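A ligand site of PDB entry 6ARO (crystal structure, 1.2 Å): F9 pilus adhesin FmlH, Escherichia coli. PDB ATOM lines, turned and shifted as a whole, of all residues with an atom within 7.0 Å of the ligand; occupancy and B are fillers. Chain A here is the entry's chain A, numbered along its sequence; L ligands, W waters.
Water W2 lies within hydrogen-bond range of the side-chain carboxylate of Asp 51 (2.7 Å), an oxygen (O5) of the ligand (2.8 Å) and the backbone carbonyl oxygen of Leu 136 (3.3 Å).
Water W1 bridges the side-chain hydroxyl of Ser 2 (3.0 Å) and the backbone carbonyl oxygen of Phe 1 (3.1 Å).
O of Ser 2 sits at hydrogen-bond distance from N of Trp 43 (2.8 Å).
OD1 of Asp 51 lies within hydrogen-bond range of N of Thr 135, 2.9 Å away.
The backbone NH (N) of Arg 142 lies within hydrogen-bond range of the backbone carbonyl oxygen (O) of Lys 132 (2.9 Å).
OD1 of Asp 45 lies within hydrogen-bond range of NE1 of Trp 43, 3.2 Å away.
The side-chain amide oxygen of Asn 140 is in hydrogen-bond range of the guanidinium group of Arg 142, 3.2 Å away.
The side-chain carboxylate (OD2) of Asp 45 sits at hydrogen-bond distance from the backbone NH (N) of Phe 1 (2.8 Å).
N of Gly 47 sits at hydrogen-bond distance from OD1 of Asn 44, at 2.9 Å.
O of Asp 53 is in hydrogen-bond range of N of Ile 94 (2.8 Å).
O3 of the ligand sits at hydrogen-bond distance from N of Asp 45.
NZ of Lys 132 is in hydrogen-bond range of O5 of the ligand (2.9 Å).
The side-chain amide nitrogen of Asn 140 is in hydrogen-bond range of an oxygen (O6) of the ligand (3.0 Å).
The side-chain carboxylate of Asp 53 lies within hydrogen-bond range of an oxygen (O3) of the ligand, at 2.5 Å.
The backbone NH (N) of Phe 1 lies within hydrogen-bond range of an oxygen (O3) of the ligand (2.9 Å).
Merely in contact with the ligand: Ser 2, Asn 44, Tyr 46, Asp 51, Ala 134 and Gly 139.
Hydrophobic or aromatic side chains within 4 Å of the ligand: Phe 1, Tyr 46 and Ala 134.
Of the 24 residues printed, 11 come within 4 Å of the ligand.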
ATOM      1  N   PHE A   1     -11.151  -3.771  14.010  1.00  0.00           N
ATOM      2  CA  PHE A   1     -10.110  -2.724  14.056  1.00  0.00           C
ATOM      3  C   PHE A   1     -10.764  -1.416  13.707  1.00  0.00           C
ATOM      4  O   PHE A   1     -11.563  -1.343  12.733  1.00  0.00           O
ATOM      5  CB  PHE A   1      -9.033  -3.060  13.014  1.00  0.00           C
ATOM      6  CG  PHE A   1      -7.984  -2.011  12.880  1.00  0.00           C
ATOM      7  CD1 PHE A   1      -7.988  -1.139  11.785  1.00  0.00           C
ATOM      8  CD2 PHE A   1      -7.010  -1.887  13.852  1.00  0.00           C
ATOM      9  CE1 PHE A   1      -7.020  -0.167  11.657  1.00  0.00           C
ATOM     10  CE2 PHE A   1      -6.027  -0.916  13.716  1.00  0.00           C
ATOM     11  CZ  PHE A   1      -6.026  -0.066  12.596  1.00  0.00           C
ATOM     12  N   SER A   2     -10.468  -0.360  14.457  1.00  0.00           N
ATOM     13  CA  SER A   2     -11.069   0.918  14.154  1.00  0.00           C
ATOM     14  C   SER A   2     -10.056   2.025  14.420  1.00  0.00           C
ATOM     15  O   SER A   2      -9.094   1.842  15.193  1.00  0.00           O
ATOM     16  CB  SER A   2     -12.305   1.175  15.006  1.00  0.00           C
ATOM     17  OG  SER A   2     -13.286   0.162  14.808  1.00  0.00           O
ATOM     18  N   SER A  10     -15.685   6.571  15.116  1.00  0.00           N
ATOM     19  CA  SER A  10     -14.884   5.425  14.681  1.00  0.00           C
ATOM     20  C   SER A  10     -14.964   5.204  13.174  1.00  0.00           C
ATOM     21  O   SER A  10     -16.012   5.387  12.551  1.00  0.00           O
ATOM     22  CB  SER A  10     -15.287   4.155  15.431  1.00  0.00           C
ATOM     23  OG  SER A  10     -16.623   3.766  15.139  1.00  0.00           O
ATOM     24  N   GLY A  12     -13.855   2.363  10.143  1.00  0.00           N
ATOM     25  CA  GLY A  12     -13.455   0.986   9.868  1.00  0.00           C
ATOM     26  C   GLY A  12     -12.836   0.746   8.498  1.00  0.00           C
ATOM     27  O   GLY A  12     -12.328  -0.334   8.256  1.00  0.00           O
ATOM     28  N   TRP A  43      -7.180   1.177  17.189  1.00  0.00           N
ATOM     29  CA  TRP A  43      -7.279   0.231  18.287  1.00  0.00           C
ATOM     30  C   TRP A  43      -7.871  -1.062  17.794  1.00  0.00           C
ATOM     31  O   TRP A  43      -8.518  -1.151  16.738  1.00  0.00           O
ATOM     32  CB  TRP A  43      -8.108   0.759  19.483  1.00  0.00           C
ATOM     33  CG  TRP A  43      -9.503   1.163  19.093  1.00  0.00           C
ATOM     34  CD1 TRP A  43     -10.602   0.362  19.133  1.00  0.00           C
ATOM     35  CD2 TRP A  43      -9.925   2.415  18.564  1.00  0.00           C
ATOM     36  NE1 TRP A  43     -11.707   1.071  18.697  1.00  0.00           N
ATOM     37  CE2 TRP A  43     -11.305   2.329  18.320  1.00  0.00           C
ATOM     38  CE3 TRP A  43      -9.265   3.608  18.263  1.00  0.00           C
ATOM     39  CZ2 TRP A  43     -12.039   3.385  17.790  1.00  0.00           C
ATOM     40  CZ3 TRP A  43     -10.006   4.666  17.721  1.00  0.00           C
ATOM     41  CH2 TRP A  43     -11.373   4.537  17.502  1.00  0.00           C
ATOM     42  N   ASN A  44      -7.617  -2.108  18.590  1.00  0.00           N
ATOM     43  CA  ASN A  44      -8.231  -3.410  18.424  1.00  0.00           C
ATOM     44  C   ASN A  44      -9.620  -3.382  19.059  1.00  0.00           C
ATOM     45  O   ASN A  44      -9.783  -2.923  20.183  1.00  0.00           O
ATOM     46  CB  ASN A  44      -7.327  -4.441  19.068  1.00  0.00           C
ATOM     47  CG  ASN A  44      -7.797  -5.823  18.868  1.00  0.00           C
ATOM     48  OD1 ASN A  44      -8.797  -6.245  19.471  1.00  0.00           O
ATOM     49  ND2 ASN A  44      -7.093  -6.566  18.033  1.00  0.00           N
ATOM     50  N   ASP A  45     -10.624  -3.885  18.341  1.00  0.00           N
ATOM     51  CA  ASP A  45     -11.996  -3.742  18.815  1.00  0.00           C
ATOM     52  C   ASP A  45     -12.364  -4.745  19.884  1.00  0.00           C
ATOM     53  O   ASP A  45     -13.381  -4.545  20.554  1.00  0.00           O
ATOM     54  CB  ASP A  45     -12.977  -3.768  17.643  1.00  0.00           C
ATOM     55  CG  ASP A  45     -13.066  -2.444  16.976  1.00  0.00           C
ATOM     56  OD1 ASP A  45     -13.352  -1.447  17.645  1.00  0.00           O
ATOM     57  OD2 ASP A  45     -12.836  -2.410  15.766  1.00  0.00           O
ATOM     58  N   TYR A  46     -11.552  -5.761  20.135  1.00  0.00           N
ATOM     59  CA  TYR A  46     -11.760  -6.664  21.273  1.00  0.00           C
ATOM     60  C   TYR A  46     -10.860  -6.358  22.444  1.00  0.00           C
ATOM     61  O   TYR A  46     -11.284  -6.511  23.608  1.00  0.00           O
ATOM     62  CB  TYR A  46     -11.486  -8.113  20.882  1.00  0.00           C
ATOM     63  CG  TYR A  46     -12.326  -8.671  19.765  1.00  0.00           C
ATOM     64  CD1 TYR A  46     -13.730  -8.702  19.838  1.00  0.00           C
ATOM     65  CD2 TYR A  46     -11.713  -9.266  18.664  1.00  0.00           C
ATOM     66  CE1 TYR A  46     -14.467  -9.256  18.803  1.00  0.00           C
ATOM     67  CE2 TYR A  46     -12.428  -9.823  17.632  1.00  0.00           C
ATOM     68  CZ  TYR A  46     -13.819  -9.808  17.724  1.00  0.00           C
ATOM     69  OH  TYR A  46     -14.571 -10.368  16.722  1.00  0.00           O
ATOM     70  N   GLY A  47      -9.606  -5.972  22.192  1.00  0.00           N
ATOM     71  CA  GLY A  47      -8.597  -5.898  23.225  1.00  0.00           C
ATOM     72  C   GLY A  47      -8.080  -7.259  23.608  1.00  0.00           C
ATOM     73  O   GLY A  47      -8.532  -8.266  23.102  1.00  0.00           O
ATOM     74  N   TYR A  50      -6.490 -10.731  21.371  1.00  0.00           N
ATOM     75  CA  TYR A  50      -7.256 -11.899  20.948  1.00  0.00           C
ATOM     76  C   TYR A  50      -7.223 -12.240  19.416  1.00  0.00           C
ATOM     77  O   TYR A  50      -6.844 -13.354  18.992  1.00  0.00           O
ATOM     78  CB  TYR A  50      -8.685 -11.788  21.532  1.00  0.00           C
ATOM     79  CG  TYR A  50      -9.620 -12.746  20.910  1.00  0.00           C
ATOM     80  CD1 TYR A  50      -9.558 -14.101  21.195  1.00  0.00           C
ATOM     81  CD2 TYR A  50     -10.572 -12.310  19.985  1.00  0.00           C
ATOM     82  CE1 TYR A  50     -10.424 -14.996  20.571  1.00  0.00           C
ATOM     83  CE2 TYR A  50     -11.443 -13.183  19.386  1.00  0.00           C
ATOM     84  CZ  TYR A  50     -11.362 -14.525  19.679  1.00  0.00           C
ATOM     85  OH  TYR A  50     -12.247 -15.393  19.055  1.00  0.00           O
ATOM     86  N   ASP A  51      -7.649 -11.282  18.610  1.00  0.00           N
ATOM     87  CA  ASP A  51      -7.622 -11.292  17.152  1.00  0.00           C
ATOM     88  C   ASP A  51      -6.764 -10.062  16.785  1.00  0.00           C
ATOM     89  O   ASP A  51      -7.284  -8.984  16.501  1.00  0.00           O
ATOM     90  CB  ASP A  51      -9.041 -11.181  16.589  1.00  0.00           C
ATOM     91  CG  ASP A  51      -9.099 -11.285  15.111  1.00  0.00           C
ATOM     92  OD1 ASP A  51      -8.058 -11.596  14.478  1.00  0.00           O
ATOM     93  OD2 ASP A  51     -10.210 -11.077  14.547  1.00  0.00           O
ATOM     94  N   THR A  52      -5.456 -10.200  16.882  1.00  0.00           N
ATOM     95  CA  THR A  52      -4.553  -9.042  16.732  1.00  0.00           C
ATOM     96  C   THR A  52      -4.616  -8.470  15.325  1.00  0.00           C
ATOM     97  O   THR A  52      -4.680  -9.201  14.317  1.00  0.00           O
ATOM     98  CB  THR A  52      -3.131  -9.508  17.059  1.00  0.00           C
ATOM     99  OG1 THR A  52      -3.093  -9.915  18.433  1.00  0.00           O
ATOM    100  CG2 THR A  52      -2.132  -8.372  16.915  1.00  0.00           C
ATOM    101  N   ASP A  53      -4.633  -7.142  15.232  1.00  0.00           N
ATOM    102  CA  ASP A  53      -4.602  -6.433  13.948  1.00  0.00           C
ATOM    103  C   ASP A  53      -3.166  -6.141  13.512  1.00  0.00           C
ATOM    104  O   ASP A  53      -2.279  -5.879  14.348  1.00  0.00           O
ATOM    105  CB  ASP A  53      -5.382  -5.144  14.078  1.00  0.00           C
ATOM    106  CG  ASP A  53      -6.853  -5.412  14.398  1.00  0.00           C
ATOM    107  OD1 ASP A  53      -7.460  -6.125  13.594  1.00  0.00           O
ATOM    108  OD2 ASP A  53      -7.328  -4.948  15.448  1.00  0.00           O
ATOM    109  N   ILE A  94      -1.566  -4.311  16.535  1.00  0.00           N
ATOM    110  CA  ILE A  94      -2.507  -3.611  17.392  1.00  0.00           C
ATOM    111  C   ILE A  94      -3.442  -4.617  18.017  1.00  0.00           C
ATOM    112  O   ILE A  94      -4.203  -5.308  17.350  1.00  0.00           O
ATOM    113  CB  ILE A  94      -3.280  -2.544  16.570  1.00  0.00           C
ATOM    114  CG1 ILE A  94      -2.291  -1.490  15.998  1.00  0.00           C
ATOM    115  CG2 ILE A  94      -4.456  -1.931  17.379  1.00  0.00           C
ATOM    116  CD1 ILE A  94      -1.826  -0.528  17.004  1.00  0.00           C
ATOM    117  N   LYS A  97      -7.428  -2.408  23.262  1.00  0.00           N
ATOM    118  CA  LYS A  97      -8.544  -1.567  22.910  1.00  0.00           C
ATOM    119  C   LYS A  97      -8.280  -0.093  23.208  1.00  0.00           C
ATOM    120  O   LYS A  97      -8.893   0.805  22.624  1.00  0.00           O
ATOM    121  CB  LYS A  97      -9.826  -2.084  23.600  1.00  0.00           C
ATOM    122  CG  LYS A  97     -11.108  -1.455  23.067  1.00  0.00           C
ATOM    123  CD  LYS A  97     -12.321  -2.307  23.438  1.00  0.00           C
ATOM    124  CE  LYS A  97     -13.624  -1.628  23.044  1.00  0.00           C
ATOM    125  NZ  LYS A  97     -14.808  -2.528  23.255  1.00  0.00           N
ATOM    126  N   LYS A 132      -5.001  -2.904   6.735  1.00  0.00           N
ATOM    127  CA  LYS A 132      -5.246  -3.687   7.936  1.00  0.00           C
ATOM    128  C   LYS A 132      -5.630  -5.119   7.592  1.00  0.00           C
ATOM    129  O   LYS A 132      -6.489  -5.318   6.728  1.00  0.00           O
ATOM    130  CB  LYS A 132      -6.415  -3.072   8.724  1.00  0.00           C
ATOM    131  CG  LYS A 132      -6.970  -3.955   9.853  1.00  0.00           C
ATOM    132  CD  LYS A 132      -8.326  -4.635   9.462  1.00  0.00           C
ATOM    133  CE  LYS A 132      -8.583  -5.802  10.414  1.00  0.00           C
ATOM    134  NZ  LYS A 132     -10.016  -6.295  10.240  1.00  0.00           N
ATOM    135  N   ILE A 133      -5.011  -6.079   8.259  1.00  0.00           N
ATOM    136  CA  ILE A 133      -5.510  -7.463   8.225  1.00  0.00           C
ATOM    137  C   ILE A 133      -5.332  -8.034   9.633  1.00  0.00           C
ATOM    138  O   ILE A 133      -4.356  -7.702  10.297  1.00  0.00           O
ATOM    139  CB  ILE A 133      -4.789  -8.281   7.131  1.00  0.00           C
ATOM    140  CG1 ILE A 133      -5.472  -9.634   6.953  1.00  0.00           C
ATOM    141  CG2 ILE A 133      -3.303  -8.473   7.463  1.00  0.00           C
ATOM    142  CD1 ILE A 133      -5.030 -10.401   5.659  1.00  0.00           C
ATOM    143  N   ALA A 134      -6.322  -8.791  10.101  1.00  0.00           N
ATOM    144  CA  ALA A 134      -6.249  -9.320  11.454  1.00  0.00           C
ATOM    145  C   ALA A 134      -5.669 -10.732  11.449  1.00  0.00           C
ATOM    146  O   ALA A 134      -4.937 -11.093  10.528  1.00  0.00           O
ATOM    147  CB  ALA A 134      -7.631  -9.221  12.141  1.00  0.00           C
ATOM    148  N   THR A 135      -6.025 -11.528  12.454  1.00  0.00           N
ATOM    149  CA  THR A 135      -5.350 -12.800  12.699  1.00  0.00           C
ATOM    150  C   THR A 135      -6.241 -14.006  12.465  1.00  0.00           C
ATOM    151  O   THR A 135      -5.783 -14.995  11.905  1.00  0.00           O
ATOM    152  CB  THR A 135      -4.787 -12.839  14.135  1.00  0.00           C
ATOM    153  OG1 THR A 135      -3.877 -11.721  14.272  1.00  0.00           O
ATOM    154  CG2 THR A 135      -3.985 -14.103  14.390  1.00  0.00           C
ATOM    155  N   LEU A 136      -7.504 -13.891  12.854  1.00  0.00           N
ATOM    156  CA  LEU A 136      -8.453 -15.013  12.788  1.00  0.00           C
ATOM    157  C   LEU A 136      -9.174 -15.006  11.463  1.00  0.00           C
ATOM    158  O   LEU A 136      -9.356 -13.962  10.832  1.00  0.00           O
ATOM    159  CB  LEU A 136      -9.461 -14.923  13.946  1.00  0.00           C
ATOM    160  CG  LEU A 136      -8.877 -14.904  15.365  1.00  0.00           C
ATOM    161  CD1 LEU A 136      -9.945 -14.829  16.480  1.00  0.00           C
ATOM    162  CD2 LEU A 136      -7.921 -16.055  15.621  1.00  0.00           C
ATOM    163  N   GLY A 139      -8.890 -12.756   8.192  1.00  0.00           N
ATOM    164  CA  GLY A 139      -8.287 -11.510   8.628  1.00  0.00           C
ATOM    165  C   GLY A 139      -9.116 -10.282   8.297  1.00  0.00           C
ATOM    166  O   GLY A 139      -8.765  -9.216   8.775  1.00  0.00           O
ATOM    167  N   ASN A 140     -10.195 -10.394   7.522  1.00  0.00           N
ATOM    168  CA  ASN A 140     -11.092  -9.257   7.288  1.00  0.00           C
ATOM    169  C   ASN A 140     -10.306  -8.010   6.867  1.00  0.00           C
ATOM    170  O   ASN A 140     -10.338  -6.978   7.529  1.00  0.00           O
ATOM    171  CB  ASN A 140     -11.973  -8.999   8.532  1.00  0.00           C
ATOM    172  CG  ASN A 140     -12.988  -7.859   8.359  1.00  0.00           C
ATOM    173  OD1 ASN A 140     -13.479  -7.564   7.260  1.00  0.00           O
ATOM    174  ND2 ASN A 140     -13.328  -7.227   9.474  1.00  0.00           N
ATOM    175  N   PRO A 141      -9.588  -8.088   5.740  1.00  0.00           N
ATOM    176  CA  PRO A 141      -8.703  -6.975   5.349  1.00  0.00           C
ATOM    177  C   PRO A 141      -9.491  -5.734   5.040  1.00  0.00           C
ATOM    178  O   PRO A 141     -10.603  -5.793   4.487  1.00  0.00           O
ATOM    179  CB  PRO A 141      -8.008  -7.492   4.085  1.00  0.00           C
ATOM    180  CG  PRO A 141      -8.939  -8.546   3.557  1.00  0.00           C
ATOM    181  CD  PRO A 141      -9.498  -9.218   4.799  1.00  0.00           C
ATOM    182  N   ARG A 142      -8.911  -4.584   5.377  1.00  0.00           N
ATOM    183  CA  ARG A 142      -9.558  -3.315   5.157  1.00  0.00           C
ATOM    184  C   ARG A 142      -8.544  -2.307   4.686  1.00  0.00           C
ATOM    185  O   ARG A 142      -7.370  -2.329   5.102  1.00  0.00           O
ATOM    186  CB  ARG A 142     -10.214  -2.779   6.462  1.00  0.00           C
ATOM    187  CG  ARG A 142     -11.275  -3.667   7.069  1.00  0.00           C
ATOM    188  CD  ARG A 142     -12.538  -3.591   6.217  1.00  0.00           C
ATOM    189  NE  ARG A 142     -13.638  -4.362   6.805  1.00  0.00           N
ATOM    190  CZ  ARG A 142     -14.434  -3.939   7.784  1.00  0.00           C
ATOM    191  NH1 ARG A 142     -14.297  -2.735   8.367  1.00  0.00           N
ATOM    192  NH2 ARG A 142     -15.411  -4.757   8.199  1.00  0.00           N
HETATM  193  C1  LIG L   1     -11.677  -8.198  13.099  1.00  0.00           C
HETATM  194  C2  LIG L   1     -16.261  -2.471  14.683  1.00  0.00           C
HETATM  195  C3  LIG L   1     -16.995  -2.105  15.781  1.00  0.00           C
HETATM  196  C4  LIG L   1     -17.074  -2.960  16.895  1.00  0.00           C
HETATM  197  C5  LIG L   1     -15.767  -6.224  17.881  1.00  0.00           C
HETATM  198  C6  LIG L   1     -16.467  -5.066  17.943  1.00  0.00           C
HETATM  199  C7  LIG L   1     -16.410  -4.172  16.867  1.00  0.00           C
HETATM  200  C8  LIG L   1     -15.678  -4.518  15.742  1.00  0.00           C
HETATM  201  C9  LIG L   1     -14.994  -5.708  15.656  1.00  0.00           C
HETATM  202  C10 LIG L   1     -15.022  -6.561  16.733  1.00  0.00           C
HETATM  203  O1  LIG L   1     -14.272  -5.980  14.486  1.00  0.00           O
HETATM  204  C11 LIG L   1     -13.258  -6.977  14.498  1.00  0.00           C
HETATM  205  C12 LIG L   1     -12.840  -7.252  13.088  1.00  0.00           C
HETATM  206  C13 LIG L   1     -10.556  -7.611  13.950  1.00  0.00           C
HETATM  207  C14 LIG L   1     -11.105  -7.320  15.331  1.00  0.00           C
HETATM  208  O2  LIG L   1     -12.184  -6.433  15.242  1.00  0.00           O
HETATM  209  C15 LIG L   1     -10.054  -6.738  16.314  1.00  0.00           C
HETATM  210  O3  LIG L   1      -9.764  -5.389  16.013  1.00  0.00           O
HETATM  211  O4  LIG L   1     -10.059  -6.423  13.319  1.00  0.00           O
HETATM  212  O5  LIG L   1     -11.259  -8.396  11.738  1.00  0.00           O
HETATM  213  O6  LIG L   1     -13.923  -7.887  12.372  1.00  0.00           O
HETATM  214  N1  LIG L   1     -15.613  -3.682  14.664  1.00  0.00           N
HETATM  215  O   HOH W   1     -14.603  -0.725  12.284  1.00  0.00           O
HETATM  216  O   HOH W   2     -10.520 -11.097  11.860  1.00  0.00           O
HETATM  217  O   HOH W   3     -14.690  -4.063  12.021  1.00  0.00           O
